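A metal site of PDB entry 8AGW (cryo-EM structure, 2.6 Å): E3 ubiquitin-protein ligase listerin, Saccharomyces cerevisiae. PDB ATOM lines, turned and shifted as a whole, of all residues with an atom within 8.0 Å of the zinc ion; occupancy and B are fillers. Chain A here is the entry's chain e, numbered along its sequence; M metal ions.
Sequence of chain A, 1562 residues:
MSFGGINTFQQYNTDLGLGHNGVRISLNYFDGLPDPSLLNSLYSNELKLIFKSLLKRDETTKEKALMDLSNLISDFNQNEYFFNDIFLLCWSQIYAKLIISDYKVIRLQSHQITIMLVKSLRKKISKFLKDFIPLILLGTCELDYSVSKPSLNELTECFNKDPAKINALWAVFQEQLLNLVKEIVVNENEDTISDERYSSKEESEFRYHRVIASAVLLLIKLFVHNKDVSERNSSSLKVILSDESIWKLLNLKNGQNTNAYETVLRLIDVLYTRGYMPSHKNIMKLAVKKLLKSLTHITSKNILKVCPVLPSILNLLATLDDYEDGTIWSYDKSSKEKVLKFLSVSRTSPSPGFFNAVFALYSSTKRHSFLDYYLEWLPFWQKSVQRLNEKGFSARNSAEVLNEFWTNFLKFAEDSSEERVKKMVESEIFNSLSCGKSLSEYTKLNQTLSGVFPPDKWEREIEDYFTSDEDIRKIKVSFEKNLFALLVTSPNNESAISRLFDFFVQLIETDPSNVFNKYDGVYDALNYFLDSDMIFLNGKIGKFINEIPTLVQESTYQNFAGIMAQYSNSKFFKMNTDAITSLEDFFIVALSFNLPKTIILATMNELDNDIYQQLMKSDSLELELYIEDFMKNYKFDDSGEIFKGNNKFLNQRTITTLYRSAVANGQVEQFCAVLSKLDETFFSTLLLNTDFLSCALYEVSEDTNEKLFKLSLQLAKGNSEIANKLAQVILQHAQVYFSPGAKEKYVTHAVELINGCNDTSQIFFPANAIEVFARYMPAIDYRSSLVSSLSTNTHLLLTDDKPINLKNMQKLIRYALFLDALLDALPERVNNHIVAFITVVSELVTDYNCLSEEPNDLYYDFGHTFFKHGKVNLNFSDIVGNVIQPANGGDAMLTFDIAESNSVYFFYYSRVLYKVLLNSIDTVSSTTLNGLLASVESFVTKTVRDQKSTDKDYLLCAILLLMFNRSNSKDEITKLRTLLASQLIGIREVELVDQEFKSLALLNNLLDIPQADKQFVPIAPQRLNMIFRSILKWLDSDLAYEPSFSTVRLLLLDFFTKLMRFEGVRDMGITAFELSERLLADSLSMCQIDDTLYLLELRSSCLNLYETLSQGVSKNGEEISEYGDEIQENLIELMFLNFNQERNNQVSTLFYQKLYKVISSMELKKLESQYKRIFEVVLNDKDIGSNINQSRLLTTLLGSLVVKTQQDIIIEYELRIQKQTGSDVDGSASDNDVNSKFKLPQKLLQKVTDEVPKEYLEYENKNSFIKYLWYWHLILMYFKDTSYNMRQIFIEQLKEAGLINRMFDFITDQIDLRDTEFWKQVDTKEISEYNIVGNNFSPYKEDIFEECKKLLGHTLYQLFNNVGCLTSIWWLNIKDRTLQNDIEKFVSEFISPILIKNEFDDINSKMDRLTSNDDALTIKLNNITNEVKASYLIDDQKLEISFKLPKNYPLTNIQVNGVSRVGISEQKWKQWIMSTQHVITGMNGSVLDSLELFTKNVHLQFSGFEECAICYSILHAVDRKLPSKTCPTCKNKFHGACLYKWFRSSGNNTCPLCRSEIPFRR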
ATOM      1  N   THR A1526     -11.798  21.962   5.477  1.00  0.00           N
ATOM      2  CA  THR A1526     -11.564  21.044   4.368  1.00  0.00           C
ATOM      3  C   THR A1526     -11.966  21.714   3.068  1.00  0.00           C
ATOM      4  O   THR A1526     -13.057  22.264   2.960  1.00  0.00           O
ATOM      5  CB  THR A1526     -12.358  19.735   4.515  1.00  0.00           C
ATOM      6  OG1 THR A1526     -13.714  20.030   4.847  1.00  0.00           O
ATOM      7  CG2 THR A1526     -11.753  18.864   5.617  1.00  0.00           C
ATOM      8  N   CYS A1527     -11.092  21.666   2.075  1.00  0.00           N
ATOM      9  CA  CYS A1527     -11.405  22.239   0.780  1.00  0.00           C
ATOM     10  C   CYS A1527     -12.520  21.440   0.121  1.00  0.00           C
ATOM     11  O   CYS A1527     -12.528  20.210   0.190  1.00  0.00           O
ATOM     12  CB  CYS A1527     -10.153  22.217  -0.086  1.00  0.00           C
ATOM     13  SG  CYS A1527     -10.303  22.827  -1.781  1.00  0.00           S
ATOM     14  N   PRO A1528     -13.501  22.116  -0.482  1.00  0.00           N
ATOM     15  CA  PRO A1528     -14.518  21.333  -1.185  1.00  0.00           C
ATOM     16  C   PRO A1528     -13.892  20.584  -2.350  1.00  0.00           C
ATOM     17  O   PRO A1528     -14.201  19.412  -2.555  1.00  0.00           O
ATOM     18  CB  PRO A1528     -15.475  22.403  -1.716  1.00  0.00           C
ATOM     19  CG  PRO A1528     -15.260  23.589  -0.835  1.00  0.00           C
ATOM     20  CD  PRO A1528     -13.811  23.564  -0.471  1.00  0.00           C
ATOM     21  N   THR A1529     -13.042  21.256  -3.110  1.00  0.00           N
ATOM     22  CA  THR A1529     -12.397  20.623  -4.263  1.00  0.00           C
ATOM     23  C   THR A1529     -11.449  19.497  -3.912  1.00  0.00           C
ATOM     24  O   THR A1529     -11.449  18.458  -4.580  1.00  0.00           O
ATOM     25  CB  THR A1529     -11.644  21.668  -5.090  1.00  0.00           C
ATOM     26  OG1 THR A1529     -12.379  22.894  -5.086  1.00  0.00           O
ATOM     27  CG2 THR A1529     -11.453  21.188  -6.523  1.00  0.00           C
ATOM     28  N   CYS A1530     -10.643  19.664  -2.869  1.00  0.00           N
ATOM     29  CA  CYS A1530      -9.650  18.642  -2.534  1.00  0.00           C
ATOM     30  C   CYS A1530      -9.775  18.132  -1.106  1.00  0.00           C
ATOM     31  O   CYS A1530     -10.127  18.888  -0.204  1.00  0.00           O
ATOM     32  CB  CYS A1530      -8.229  19.121  -2.855  1.00  0.00           C
ATOM     33  SG  CYS A1530      -7.570  20.465  -1.841  1.00  0.00           S
ATOM     34  N   LYS A1531      -9.455  16.871  -0.891  1.00  0.00           N
ATOM     35  CA  LYS A1531      -9.616  16.262   0.434  1.00  0.00           C
ATOM     36  C   LYS A1531      -8.664  16.813   1.492  1.00  0.00           C
ATOM     37  O   LYS A1531      -8.860  16.565   2.685  1.00  0.00           O
ATOM     38  CB  LYS A1531      -9.463  14.740   0.343  1.00  0.00           C
ATOM     39  CG  LYS A1531     -10.485  14.071  -0.549  1.00  0.00           C
ATOM     40  CD  LYS A1531     -10.277  12.569  -0.600  1.00  0.00           C
ATOM     41  CE  LYS A1531     -11.300  11.893  -1.504  1.00  0.00           C
ATOM     42  NZ  LYS A1531     -11.088  10.429  -1.594  1.00  0.00           N
ATOM     43  N   ASN A1532      -7.637  17.547   1.073  1.00  0.00           N
ATOM     44  CA  ASN A1532      -6.636  18.014   2.027  1.00  0.00           C
ATOM     45  C   ASN A1532      -7.230  18.866   3.137  1.00  0.00           C
ATOM     46  O   ASN A1532      -8.121  19.676   2.907  1.00  0.00           O
ATOM     47  CB  ASN A1532      -5.557  18.797   1.285  1.00  0.00           C
ATOM     48  CG  ASN A1532      -4.897  17.969   0.195  1.00  0.00           C
ATOM     49  OD1 ASN A1532      -5.265  18.059  -0.969  1.00  0.00           O
ATOM     50  ND2 ASN A1532      -3.929  17.146   0.582  1.00  0.00           N
ATOM     51  N   PHE A1534      -6.920  21.720   6.102  1.00  0.00           N
ATOM     52  CA  PHE A1534      -6.125  22.898   6.425  1.00  0.00           C
ATOM     53  C   PHE A1534      -6.499  23.442   7.782  1.00  0.00           C
ATOM     54  O   PHE A1534      -7.674  23.457   8.135  1.00  0.00           O
ATOM     55  CB  PHE A1534      -6.359  24.010   5.400  1.00  0.00           C
ATOM     56  CG  PHE A1534      -6.173  23.578   3.972  1.00  0.00           C
ATOM     57  CD1 PHE A1534      -4.924  23.609   3.388  1.00  0.00           C
ATOM     58  CD2 PHE A1534      -7.257  23.179   3.208  1.00  0.00           C
ATOM     59  CE1 PHE A1534      -4.739  23.231   2.077  1.00  0.00           C
ATOM     60  CE2 PHE A1534      -7.079  22.797   1.892  1.00  0.00           C
ATOM     61  CZ  PHE A1534      -5.828  22.826   1.325  1.00  0.00           C
ATOM     62  N   LEU A1539      -5.183  28.561   6.611  1.00  0.00           N
ATOM     63  CA  LEU A1539      -5.980  28.813   5.422  1.00  0.00           C
ATOM     64  C   LEU A1539      -6.328  30.280   5.294  1.00  0.00           C
ATOM     65  O   LEU A1539      -6.239  30.851   4.213  1.00  0.00           O
ATOM     66  CB  LEU A1539      -7.263  27.991   5.460  1.00  0.00           C
ATOM     67  CG  LEU A1539      -8.044  27.893   4.160  1.00  0.00           C
ATOM     68  CD1 LEU A1539      -7.184  27.252   3.088  1.00  0.00           C
ATOM     69  CD2 LEU A1539      -9.323  27.100   4.370  1.00  0.00           C
ATOM     70  N   THR A1550      -8.999  31.440  -2.151  1.00  0.00           N
ATOM     71  CA  THR A1550      -8.319  30.538  -3.069  1.00  0.00           C
ATOM     72  C   THR A1550      -7.544  29.458  -2.332  1.00  0.00           C
ATOM     73  O   THR A1550      -6.736  29.758  -1.466  1.00  0.00           O
ATOM     74  CB  THR A1550      -7.338  31.314  -3.977  1.00  0.00           C
ATOM     75  OG1 THR A1550      -6.528  32.176  -3.167  1.00  0.00           O
ATOM     76  CG2 THR A1550      -8.091  32.145  -4.999  1.00  0.00           C
ATOM     77  N   CYS A1551      -7.790  28.203  -2.685  1.00  0.00           N
ATOM     78  CA  CYS A1551      -7.090  27.096  -2.032  1.00  0.00           C
ATOM     79  C   CYS A1551      -5.600  27.129  -2.362  1.00  0.00           C
ATOM     80  O   CYS A1551      -5.223  27.370  -3.504  1.00  0.00           O
ATOM     81  CB  CYS A1551      -7.693  25.782  -2.493  1.00  0.00           C
ATOM     82  SG  CYS A1551      -6.924  24.277  -1.870  1.00  0.00           S
ATOM     83  N   PRO A1552      -4.742  26.912  -1.357  1.00  0.00           N
ATOM     84  CA  PRO A1552      -3.321  26.853  -1.684  1.00  0.00           C
ATOM     85  C   PRO A1552      -2.951  25.682  -2.586  1.00  0.00           C
ATOM     86  O   PRO A1552      -2.225  25.860  -3.562  1.00  0.00           O
ATOM     87  CB  PRO A1552      -2.640  26.676  -0.322  1.00  0.00           C
ATOM     88  CG  PRO A1552      -3.673  27.001   0.698  1.00  0.00           C
ATOM     89  CD  PRO A1552      -4.997  26.720   0.080  1.00  0.00           C
ATOM     90  N   LEU A1553      -3.437  24.493  -2.245  1.00  0.00           N
ATOM     91  CA  LEU A1553      -3.118  23.297  -3.028  1.00  0.00           C
ATOM     92  C   LEU A1553      -3.700  23.271  -4.431  1.00  0.00           C
ATOM     93  O   LEU A1553      -3.040  22.840  -5.374  1.00  0.00           O
ATOM     94  CB  LEU A1553      -3.457  22.020  -2.274  1.00  0.00           C
ATOM     95  CG  LEU A1553      -2.436  21.641  -1.198  1.00  0.00           C
ATOM     96  CD1 LEU A1553      -2.385  20.133  -1.065  1.00  0.00           C
ATOM     97  CD2 LEU A1553      -1.049  22.167  -1.568  1.00  0.00           C
ATOM     98  N   CYS A1554      -4.939  23.727  -4.575  1.00  0.00           N
ATOM     99  CA  CYS A1554      -5.598  23.627  -5.878  1.00  0.00           C
ATOM    100  C   CYS A1554      -6.153  24.960  -6.341  1.00  0.00           C
ATOM    101  O   CYS A1554      -6.448  25.840  -5.549  1.00  0.00           O
ATOM    102  CB  CYS A1554      -6.701  22.566  -5.851  1.00  0.00           C
ATOM    103  SG  CYS A1554      -8.238  23.073  -5.041  1.00  0.00           S
ATOM    104  N   ARG A1555      -6.291  25.116  -7.650  1.00  0.00           N
ATOM    105  CA  ARG A1555      -6.781  26.374  -8.208  1.00  0.00           C
ATOM    106  C   ARG A1555      -8.197  26.719  -7.768  1.00  0.00           C
ATOM    107  O   ARG A1555      -8.500  27.889  -7.530  1.00  0.00           O
ATOM    108  CB  ARG A1555      -6.702  26.360  -9.745  1.00  0.00           C
ATOM    109  CG  ARG A1555      -5.348  26.763 -10.302  1.00  0.00           C
ATOM    110  CD  ARG A1555      -4.342  25.621 -10.226  1.00  0.00           C
ATOM    111  NE  ARG A1555      -2.969  26.103 -10.298  1.00  0.00           N
ATOM    112  CZ  ARG A1555      -2.212  26.363  -9.239  1.00  0.00           C
ATOM    113  NH1 ARG A1555      -2.698  26.195  -8.014  1.00  0.00           N
ATOM    114  NH2 ARG A1555      -0.971  26.807  -9.397  1.00  0.00           N
ATOM    115  N   SER A1556      -9.070  25.721  -7.662  1.00  0.00           N
ATOM    116  CA  SER A1556     -10.470  25.998  -7.348  1.00  0.00           C
ATOM    117  C   SER A1556     -10.713  26.668  -5.996  1.00  0.00           C
ATOM    118  O   SER A1556     -10.033  26.379  -5.020  1.00  0.00           O
ATOM    119  CB  SER A1556     -11.304  24.726  -7.474  1.00  0.00           C
ATOM    120  OG  SER A1556     -12.662  24.975  -7.140  1.00  0.00           O
ATOM    121  N   GLU A1557     -11.685  27.566  -5.957  1.00  0.00           N
ATOM    122  CA  GLU A1557     -11.979  28.324  -4.741  1.00  0.00           C
ATOM    123  C   GLU A1557     -12.621  27.598  -3.569  1.00  0.00           C
ATOM    124  O   GLU A1557     -13.305  26.592  -3.766  1.00  0.00           O
ATOM    125  CB  GLU A1557     -12.857  29.527  -5.103  1.00  0.00           C
ATOM    126  N   ILE A1558     -12.397  28.097  -2.363  1.00  0.00           N
ATOM    127  CA  ILE A1558     -13.022  27.519  -1.181  1.00  0.00           C
ATOM    128  C   ILE A1558     -14.015  28.548  -0.657  1.00  0.00           C
ATOM    129  O   ILE A1558     -13.645  29.700  -0.446  1.00  0.00           O
ATOM    130  CB  ILE A1558     -12.005  27.258  -0.059  1.00  0.00           C
ATOM    131  CG1 ILE A1558     -10.880  26.347  -0.542  1.00  0.00           C
ATOM    132  CG2 ILE A1558     -12.672  26.676   1.172  1.00  0.00           C
ATOM    133  CD1 ILE A1558      -9.889  26.005   0.548  1.00  0.00           C
HETATM  134 ZN    ZN M   1      -8.194  22.530  -2.757  1.00  0.00          ZN
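N of Leu 1553 lies close to SG of Cys 1551 (3.5 Å).
SG of Cys 1527 lies close to N of Thr 1529, at 3.4 Å.
SG of Cys 1530 lies close to OD1 of Asn 1532 (3.4 Å).
The side-chain sulfur (SG) of Cys 1554 lies close to the backbone carbonyl oxygen (O) of Ser 1556 (3.8 Å).
Four residues have an atom within 4 Å of the zinc ion: Cys 1527, Cys 1530, Cys 1551 and Cys 1554.
The nearest printed residue that does not touch the zinc ion is Thr 1529 (4.3 Å).
The zinc ion is bound by the side-chain sulfur (SG) of Cys 1551 (2.3 Å), the side-chain sulfur (SG) of Cys 1527 (2.3 Å), the side-chain sulfur (SG) of Cys 1530 (2.3 Å) and the side-chain sulfur (SG) of Cys 1554 (2.3 Å).
The zinc ion has four donor atoms within binding distance.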
